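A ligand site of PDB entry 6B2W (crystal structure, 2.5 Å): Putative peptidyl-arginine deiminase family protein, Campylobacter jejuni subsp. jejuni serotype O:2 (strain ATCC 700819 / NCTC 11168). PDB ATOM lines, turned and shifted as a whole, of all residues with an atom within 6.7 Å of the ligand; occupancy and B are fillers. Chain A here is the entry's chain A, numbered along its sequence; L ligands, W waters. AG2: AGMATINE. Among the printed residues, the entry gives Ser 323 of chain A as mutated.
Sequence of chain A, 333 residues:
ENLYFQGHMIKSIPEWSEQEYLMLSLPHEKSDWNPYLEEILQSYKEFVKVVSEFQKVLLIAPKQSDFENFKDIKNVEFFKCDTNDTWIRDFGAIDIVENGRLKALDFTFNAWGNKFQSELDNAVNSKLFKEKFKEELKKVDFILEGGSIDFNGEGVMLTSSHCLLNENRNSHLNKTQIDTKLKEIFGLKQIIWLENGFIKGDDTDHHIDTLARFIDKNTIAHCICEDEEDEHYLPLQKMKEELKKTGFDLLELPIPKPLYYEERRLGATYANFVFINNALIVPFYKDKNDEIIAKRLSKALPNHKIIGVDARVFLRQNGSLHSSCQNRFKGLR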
ATOM      1  N   ASP A  32     -11.796 -22.716 -26.534  1.00  0.00           N
ATOM      2  CA  ASP A  32     -12.889 -23.023 -25.608  1.00  0.00           C
ATOM      3  C   ASP A  32     -13.598 -21.761 -25.070  1.00  0.00           C
ATOM      4  O   ASP A  32     -14.597 -21.865 -24.360  1.00  0.00           O
ATOM      5  CB  ASP A  32     -12.378 -23.863 -24.437  1.00  0.00           C
ATOM      6  CG  ASP A  32     -12.006 -25.288 -24.850  1.00  0.00           C
ATOM      7  OD1 ASP A  32     -12.342 -25.695 -25.976  1.00  0.00           O
ATOM      8  OD2 ASP A  32     -11.358 -25.999 -24.044  1.00  0.00           O
ATOM      9  N   ASP A  85      -5.112 -22.781 -26.920  1.00  0.00           N
ATOM     10  CA  ASP A  85      -5.735 -22.044 -25.817  1.00  0.00           C
ATOM     11  C   ASP A  85      -4.885 -20.831 -25.382  1.00  0.00           C
ATOM     12  O   ASP A  85      -3.881 -20.495 -26.020  1.00  0.00           O
ATOM     13  CB  ASP A  85      -5.975 -22.993 -24.643  1.00  0.00           C
ATOM     14  CG  ASP A  85      -7.208 -22.624 -23.823  1.00  0.00           C
ATOM     15  OD1 ASP A  85      -7.708 -21.489 -23.950  1.00  0.00           O
ATOM     16  OD2 ASP A  85      -7.673 -23.479 -23.048  1.00  0.00           O
ATOM     17  N   TRP A  87      -3.692 -20.064 -22.068  1.00  0.00           N
ATOM     18  CA  TRP A  87      -3.001 -20.176 -20.778  1.00  0.00           C
ATOM     19  C   TRP A  87      -1.490 -20.260 -20.979  1.00  0.00           C
ATOM     20  O   TRP A  87      -0.873 -21.307 -20.774  1.00  0.00           O
ATOM     21  CB  TRP A  87      -3.531 -21.376 -20.003  1.00  0.00           C
ATOM     22  CG  TRP A  87      -5.023 -21.372 -19.874  1.00  0.00           C
ATOM     23  CD1 TRP A  87      -5.907 -22.200 -20.506  1.00  0.00           C
ATOM     24  CD2 TRP A  87      -5.816 -20.485 -19.077  1.00  0.00           C
ATOM     25  NE1 TRP A  87      -7.192 -21.890 -20.141  1.00  0.00           N
ATOM     26  CE2 TRP A  87      -7.161 -20.833 -19.270  1.00  0.00           C
ATOM     27  CE3 TRP A  87      -5.508 -19.422 -18.225  1.00  0.00           C
ATOM     28  CZ2 TRP A  87      -8.203 -20.166 -18.631  1.00  0.00           C
ATOM     29  CZ3 TRP A  87      -6.555 -18.745 -17.595  1.00  0.00           C
ATOM     30  CH2 TRP A  87      -7.884 -19.134 -17.803  1.00  0.00           C
ATOM     31  N   ARG A  89       0.968 -19.000 -19.289  1.00  0.00           N
ATOM     32  CA  ARG A  89       1.735 -19.291 -18.078  1.00  0.00           C
ATOM     33  C   ARG A  89       2.283 -20.718 -18.086  1.00  0.00           C
ATOM     34  O   ARG A  89       3.372 -20.969 -17.591  1.00  0.00           O
ATOM     35  CB  ARG A  89       0.866 -19.090 -16.836  1.00  0.00           C
ATOM     36  CG  ARG A  89       1.530 -19.410 -15.504  1.00  0.00           C
ATOM     37  CD  ARG A  89       2.794 -18.607 -15.248  1.00  0.00           C
ATOM     38  NE  ARG A  89       2.537 -17.160 -15.253  1.00  0.00           N
ATOM     39  CZ  ARG A  89       3.460 -16.230 -15.050  1.00  0.00           C
ATOM     40  NH1 ARG A  89       4.724 -16.566 -14.804  1.00  0.00           N
ATOM     41  NH2 ARG A  89       3.116 -14.954 -15.070  1.00  0.00           N
ATOM     42  N   ASP A  90       1.516 -21.640 -18.661  1.00  0.00           N
ATOM     43  CA  ASP A  90       1.828 -23.060 -18.599  1.00  0.00           C
ATOM     44  C   ASP A  90       2.597 -23.599 -19.805  1.00  0.00           C
ATOM     45  O   ASP A  90       3.303 -24.600 -19.689  1.00  0.00           O
ATOM     46  CB  ASP A  90       0.530 -23.848 -18.405  1.00  0.00           C
ATOM     47  CG  ASP A  90      -0.188 -23.483 -17.106  1.00  0.00           C
ATOM     48  OD1 ASP A  90       0.481 -22.934 -16.201  1.00  0.00           O
ATOM     49  OD2 ASP A  90      -1.395 -23.746 -16.990  1.00  0.00           O
ATOM     50  N   TRP A 112      -1.857 -30.481 -19.214  1.00  0.00           N
ATOM     51  CA  TRP A 112      -2.248 -30.944 -17.872  1.00  0.00           C
ATOM     52  C   TRP A 112      -2.661 -32.421 -17.824  1.00  0.00           C
ATOM     53  O   TRP A 112      -3.595 -32.798 -17.108  1.00  0.00           O
ATOM     54  CB  TRP A 112      -3.369 -30.047 -17.321  1.00  0.00           C
ATOM     55  CG  TRP A 112      -3.114 -28.590 -17.599  1.00  0.00           C
ATOM     56  CD1 TRP A 112      -2.198 -27.788 -16.986  1.00  0.00           C
ATOM     57  CD2 TRP A 112      -3.753 -27.775 -18.592  1.00  0.00           C
ATOM     58  NE1 TRP A 112      -2.231 -26.521 -17.516  1.00  0.00           N
ATOM     59  CE2 TRP A 112      -3.175 -26.485 -18.506  1.00  0.00           C
ATOM     60  CE3 TRP A 112      -4.761 -27.999 -19.536  1.00  0.00           C
ATOM     61  CZ2 TRP A 112      -3.574 -25.430 -19.329  1.00  0.00           C
ATOM     62  CZ3 TRP A 112      -5.156 -26.953 -20.349  1.00  0.00           C
ATOM     63  CH2 TRP A 112      -4.567 -25.680 -20.244  1.00  0.00           C
ATOM     64  N   PHE A 116      -6.745 -31.627 -22.743  1.00  0.00           N
ATOM     65  CA  PHE A 116      -7.141 -30.928 -23.968  1.00  0.00           C
ATOM     66  C   PHE A 116      -6.040 -31.079 -25.023  1.00  0.00           C
ATOM     67  O   PHE A 116      -4.988 -31.666 -24.748  1.00  0.00           O
ATOM     68  CB  PHE A 116      -7.410 -29.445 -23.680  1.00  0.00           C
ATOM     69  CG  PHE A 116      -8.542 -29.213 -22.720  1.00  0.00           C
ATOM     70  CD1 PHE A 116      -9.851 -29.150 -23.176  1.00  0.00           C
ATOM     71  CD2 PHE A 116      -8.305 -29.056 -21.357  1.00  0.00           C
ATOM     72  CE1 PHE A 116     -10.904 -28.940 -22.298  1.00  0.00           C
ATOM     73  CE2 PHE A 116      -9.351 -28.838 -20.476  1.00  0.00           C
ATOM     74  CZ  PHE A 116     -10.651 -28.781 -20.941  1.00  0.00           C
ATOM     75  N   GLU A 145       4.683 -27.208 -16.510  1.00  0.00           N
ATOM     76  CA  GLU A 145       3.963 -25.940 -16.676  1.00  0.00           C
ATOM     77  C   GLU A 145       4.562 -24.896 -15.730  1.00  0.00           C
ATOM     78  O   GLU A 145       4.865 -25.197 -14.578  1.00  0.00           O
ATOM     79  CB  GLU A 145       2.475 -26.112 -16.360  1.00  0.00           C
ATOM     80  CG  GLU A 145       1.762 -27.180 -17.166  1.00  0.00           C
ATOM     81  CD  GLU A 145       1.782 -28.542 -16.500  1.00  0.00           C
ATOM     82  OE1 GLU A 145       1.516 -28.603 -15.281  1.00  0.00           O
ATOM     83  OE2 GLU A 145       2.055 -29.549 -17.180  1.00  0.00           O
ATOM     84  N   GLY A 147       3.060 -22.450 -14.323  1.00  0.00           N
ATOM     85  CA  GLY A 147       2.144 -22.227 -13.210  1.00  0.00           C
ATOM     86  C   GLY A 147       2.327 -23.180 -12.029  1.00  0.00           C
ATOM     87  O   GLY A 147       1.840 -22.899 -10.937  1.00  0.00           O
ATOM     88  N   SER A 148       3.007 -24.297 -12.247  1.00  0.00           N
ATOM     89  CA  SER A 148       3.198 -25.301 -11.187  1.00  0.00           C
ATOM     90  C   SER A 148       4.393 -25.005 -10.277  1.00  0.00           C
ATOM     91  O   SER A 148       4.573 -25.698  -9.278  1.00  0.00           O
ATOM     92  CB  SER A 148       3.341 -26.702 -11.794  1.00  0.00           C
ATOM     93  OG  SER A 148       4.541 -26.836 -12.528  1.00  0.00           O
ATOM     94  N   GLY A 201     -12.496 -26.321  -8.806  1.00  0.00           N
ATOM     95  CA  GLY A 201     -12.651 -25.750 -10.141  1.00  0.00           C
ATOM     96  C   GLY A 201     -11.340 -25.830 -10.886  1.00  0.00           C
ATOM     97  O   GLY A 201     -11.317 -25.813 -12.118  1.00  0.00           O
ATOM     98  N   ASP A 202     -10.236 -25.909 -10.141  1.00  0.00           N
ATOM     99  CA  ASP A 202      -8.915 -26.074 -10.723  1.00  0.00           C
ATOM    100  C   ASP A 202      -8.801 -27.462 -11.365  1.00  0.00           C
ATOM    101  O   ASP A 202      -8.913 -28.476 -10.684  1.00  0.00           O
ATOM    102  CB  ASP A 202      -7.840 -25.909  -9.642  1.00  0.00           C
ATOM    103  CG  ASP A 202      -6.445 -25.776 -10.199  1.00  0.00           C
ATOM    104  OD1 ASP A 202      -6.237 -25.038 -11.188  1.00  0.00           O
ATOM    105  OD2 ASP A 202      -5.538 -26.403  -9.618  1.00  0.00           O
ATOM    106  N   ASP A 203      -8.584 -27.479 -12.679  1.00  0.00           N
ATOM    107  CA  ASP A 203      -8.480 -28.725 -13.443  1.00  0.00           C
ATOM    108  C   ASP A 203      -7.040 -29.036 -13.831  1.00  0.00           C
ATOM    109  O   ASP A 203      -6.790 -29.789 -14.781  1.00  0.00           O
ATOM    110  CB  ASP A 203      -9.367 -28.650 -14.694  1.00  0.00           C
ATOM    111  CG  ASP A 203      -8.975 -27.519 -15.621  1.00  0.00           C
ATOM    112  OD1 ASP A 203      -7.772 -27.203 -15.750  1.00  0.00           O
ATOM    113  OD2 ASP A 203      -9.878 -26.930 -16.229  1.00  0.00           O
ATOM    114  N   THR A 204      -6.093 -28.469 -13.097  1.00  0.00           N
ATOM    115  CA  THR A 204      -4.678 -28.552 -13.440  1.00  0.00           C
ATOM    116  C   THR A 204      -3.914 -29.455 -12.469  1.00  0.00           C
ATOM    117  O   THR A 204      -2.690 -29.568 -12.565  1.00  0.00           O
ATOM    118  CB  THR A 204      -4.064 -27.130 -13.448  1.00  0.00           C
ATOM    119  OG1 THR A 204      -2.865 -27.124 -14.241  1.00  0.00           O
ATOM    120  CG2 THR A 204      -3.740 -26.675 -12.058  1.00  0.00           C
ATOM    121  N   HIS A 207      -2.097 -26.691  -9.083  1.00  0.00           N
ATOM    122  CA  HIS A 207      -0.992 -25.773  -9.384  1.00  0.00           C
ATOM    123  C   HIS A 207      -0.668 -24.857  -8.213  1.00  0.00           C
ATOM    124  O   HIS A 207      -1.569 -24.290  -7.606  1.00  0.00           O
ATOM    125  CB  HIS A 207      -1.335 -24.879 -10.565  1.00  0.00           C
ATOM    126  CG  HIS A 207      -0.833 -25.374 -11.876  1.00  0.00           C
ATOM    127  ND1 HIS A 207      -0.760 -24.574 -12.984  1.00  0.00           N
ATOM    128  CD2 HIS A 207      -0.363 -26.588 -12.255  1.00  0.00           C
ATOM    129  CE1 HIS A 207      -0.274 -25.262 -14.002  1.00  0.00           C
ATOM    130  NE2 HIS A 207      -0.024 -26.485 -13.587  1.00  0.00           N
ATOM    131  N   ASP A 209       0.442 -21.947  -8.251  1.00  0.00           N
ATOM    132  CA  ASP A 209       0.045 -20.543  -8.476  1.00  0.00           C
ATOM    133  C   ASP A 209      -1.426 -20.248  -8.159  1.00  0.00           C
ATOM    134  O   ASP A 209      -1.885 -19.116  -8.350  1.00  0.00           O
ATOM    135  CB  ASP A 209       0.442 -20.074  -9.889  1.00  0.00           C
ATOM    136  CG  ASP A 209      -0.542 -20.516 -10.980  1.00  0.00           C
ATOM    137  OD1 ASP A 209      -1.380 -21.410 -10.758  1.00  0.00           O
ATOM    138  OD2 ASP A 209      -0.454 -19.925 -12.079  1.00  0.00           O
ATOM    139  N   THR A 210      -2.161 -21.248  -7.688  1.00  0.00           N
ATOM    140  CA  THR A 210      -3.500 -21.045  -7.124  1.00  0.00           C
ATOM    141  C   THR A 210      -3.500 -21.119  -5.598  1.00  0.00           C
ATOM    142  O   THR A 210      -4.527 -20.873  -4.966  1.00  0.00           O
ATOM    143  CB  THR A 210      -4.509 -22.078  -7.650  1.00  0.00           C
ATOM    144  OG1 THR A 210      -4.124 -23.393  -7.236  1.00  0.00           O
ATOM    145  CG2 THR A 210      -4.596 -22.034  -9.177  1.00  0.00           C
ATOM    146  N   ASN A 272      -3.368 -16.043  -7.627  1.00  0.00           N
ATOM    147  CA  ASN A 272      -3.070 -15.995  -9.059  1.00  0.00           C
ATOM    148  C   ASN A 272      -2.831 -14.558  -9.560  1.00  0.00           C
ATOM    149  O   ASN A 272      -3.370 -14.165 -10.596  1.00  0.00           O
ATOM    150  CB  ASN A 272      -4.197 -16.686  -9.838  1.00  0.00           C
ATOM    151  CG  ASN A 272      -3.704 -17.344 -11.118  1.00  0.00           C
ATOM    152  OD1 ASN A 272      -3.935 -16.844 -12.211  1.00  0.00           O
ATOM    153  ND2 ASN A 272      -3.027 -18.472 -10.977  1.00  0.00           N
ATOM    154  N   GLN A 317     -13.000 -20.910 -17.497  1.00  0.00           N
ATOM    155  CA  GLN A 317     -12.077 -21.904 -18.040  1.00  0.00           C
ATOM    156  C   GLN A 317     -10.977 -22.250 -17.033  1.00  0.00           C
ATOM    157  O   GLN A 317      -9.886 -22.667 -17.413  1.00  0.00           O
ATOM    158  CB  GLN A 317     -11.507 -21.418 -19.376  1.00  0.00           C
ATOM    159  CG  GLN A 317     -12.533 -21.339 -20.498  1.00  0.00           C
ATOM    160  CD  GLN A 317     -13.089 -22.697 -20.901  1.00  0.00           C
ATOM    161  OE1 GLN A 317     -12.429 -23.729 -20.737  1.00  0.00           O
ATOM    162  NE2 GLN A 317     -14.299 -22.706 -21.433  1.00  0.00           N
ATOM    163  N   ASN A 318     -11.280 -22.064 -15.747  1.00  0.00           N
ATOM    164  CA  ASN A 318     -10.504 -22.602 -14.608  1.00  0.00           C
ATOM    165  C   ASN A 318      -9.101 -22.040 -14.356  1.00  0.00           C
ATOM    166  O   ASN A 318      -8.283 -22.670 -13.679  1.00  0.00           O
ATOM    167  CB  ASN A 318     -10.475 -24.121 -14.700  1.00  0.00           C
ATOM    168  CG  ASN A 318     -11.867 -24.726 -14.823  1.00  0.00           C
ATOM    169  OD1 ASN A 318     -12.784 -24.327 -14.113  1.00  0.00           O
ATOM    170  ND2 ASN A 318     -12.024 -25.669 -15.739  1.00  0.00           N
ATOM    171  N   GLY A 319      -8.829 -20.837 -14.870  1.00  0.00           N
ATOM    172  CA  GLY A 319      -7.591 -20.115 -14.560  1.00  0.00           C
ATOM    173  C   GLY A 319      -7.884 -18.684 -14.183  1.00  0.00           C
ATOM    174  O   GLY A 319      -9.043 -18.268 -14.177  1.00  0.00           O
ATOM    175  N   SER A 320      -6.855 -17.928 -13.834  1.00  0.00           N
ATOM    176  CA  SER A 320      -7.004 -16.510 -13.535  1.00  0.00           C
ATOM    177  C   SER A 320      -5.867 -15.705 -14.180  1.00  0.00           C
ATOM    178  O   SER A 320      -5.293 -16.138 -15.178  1.00  0.00           O
ATOM    179  CB  SER A 320      -7.082 -16.295 -12.025  1.00  0.00           C
ATOM    180  OG  SER A 320      -7.545 -14.991 -11.713  1.00  0.00           O
ATOM    181  N   HIS A 322      -2.633 -14.691 -13.469  1.00  0.00           N
ATOM    182  CA  HIS A 322      -1.281 -15.241 -13.564  1.00  0.00           C
ATOM    183  C   HIS A 322      -1.208 -16.352 -14.610  1.00  0.00           C
ATOM    184  O   HIS A 322      -0.292 -16.388 -15.432  1.00  0.00           O
ATOM    185  CB  HIS A 322      -0.818 -15.760 -12.213  1.00  0.00           C
ATOM    186  CG  HIS A 322       0.633 -16.125 -12.164  1.00  0.00           C
ATOM    187  ND1 HIS A 322       1.063 -17.427 -12.069  1.00  0.00           N
ATOM    188  CD2 HIS A 322       1.745 -15.363 -12.181  1.00  0.00           C
ATOM    189  CE1 HIS A 322       2.388 -17.453 -12.038  1.00  0.00           C
ATOM    190  NE2 HIS A 322       2.821 -16.211 -12.101  1.00  0.00           N
ATOM    191  N   SER A 323      -2.184 -17.246 -14.569  1.00  0.00           N
ATOM    192  CA  SER A 323      -2.369 -18.288 -15.580  1.00  0.00           C
ATOM    193  C   SER A 323      -2.390 -17.769 -17.022  1.00  0.00           C
ATOM    194  O   SER A 323      -1.957 -18.452 -17.946  1.00  0.00           O
ATOM    195  CB  SER A 323      -3.685 -19.008 -15.316  1.00  0.00           C
ATOM    196  OG  SER A 323      -3.719 -19.556 -14.002  1.00  0.00           O
ATOM    197  N   SER A 324      -2.917 -16.564 -17.224  1.00  0.00           N
ATOM    198  CA  SER A 324      -3.109 -16.001 -18.558  1.00  0.00           C
ATOM    199  C   SER A 324      -1.964 -15.130 -19.045  1.00  0.00           C
ATOM    200  O   SER A 324      -2.129 -14.380 -20.000  1.00  0.00           O
ATOM    201  CB  SER A 324      -4.405 -15.187 -18.582  1.00  0.00           C
ATOM    202  OG  SER A 324      -5.498 -15.965 -18.130  1.00  0.00           O
HETATM  203  N   AG2 L   1      -8.966 -25.242 -19.914  1.00  0.00           N
HETATM  204  CA  AG2 L   1      -8.613 -25.561 -18.528  1.00  0.00           C
HETATM  205  CB  AG2 L   1      -7.221 -25.010 -18.177  1.00  0.00           C
HETATM  206  CG  AG2 L   1      -7.253 -24.288 -16.819  1.00  0.00           C
HETATM  207  CD  AG2 L   1      -6.041 -23.369 -16.697  1.00  0.00           C
HETATM  208  NE  AG2 L   1      -5.161 -23.818 -15.605  1.00  0.00           N
HETATM  209  CZ  AG2 L   1      -4.042 -23.171 -15.248  1.00  0.00           C
HETATM  210  NH1 AG2 L   1      -3.288 -23.633 -14.254  1.00  0.00           N
HETATM  211  NH2 AG2 L   1      -3.638 -22.079 -15.900  1.00  0.00           N
HETATM  212  O   HOH W   1      -1.319 -21.380 -14.376  1.00  0.00           O
HETATM  213  O   HOH W   2      -9.888 -24.305 -22.148  1.00  0.00           O
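Residues that only touch the ligand: Trp 87, Trp 112, Phe 116, Asp 203, Thr 204, Gln 317 and Asn 318.
The side-chain amide nitrogen (ND2) of Asn 318 sits at hydrogen-bond distance from the side-chain carboxylate (OD2) of Asp 203 (2.5 Å).
The side-chain hydroxyl (OG1) of Thr 210 is in hydrogen-bond range of the backbone carbonyl oxygen (O) of His 207.
NE2 of His 207 sits at hydrogen-bond distance from OE1 of Glu 145, at 3.1 Å.
O of Ser 323 sits close to N of Arg 89.
The backbone NH (N) of Ser 323 sits at hydrogen-bond distance from the side-chain amide oxygen (OD1) of Asn 272 (3.0 Å).
The side-chain amide nitrogen (NE2) of Gln 317 lies within hydrogen-bond range of the backbone carbonyl oxygen (O) of Asp 32 (3.1 Å).
NE1 of Trp 112 sits close to OG1 of Thr 204 (3.4 Å).
The side-chain amide oxygen (OD1) of Asn 318 sits close to the backbone carbonyl oxygen (O) of Gly 201 (2.9 Å).
Water W1 lies within hydrogen-bond range of the side-chain carboxylate (OD2) of Asp 209 (2.9 Å), a nitrogen (NH2) of the ligand (2.9 Å), the side-chain carboxylate (OD1) of Asp 90 (3.0 Å) and the side-chain hydroxyl (OG) of Ser 323 (3.0 Å).
A ring nitrogen (ND1) of His 207 is in hydrogen-bond range of a nitrogen (NH1) of the ligand, at 3.0 Å.
NH2 of the ligand lies within salt-bridge range of OD2 of Asp 90 (3.0 Å).
The side-chain hydroxyl of Ser 323 lies close to a nitrogen (NH2) of the ligand (3.2 Å).
A nitrogen (N) of the ligand lies within salt-bridge range of the side-chain carboxylate (OD2) of Asp 85 (3.8 Å).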
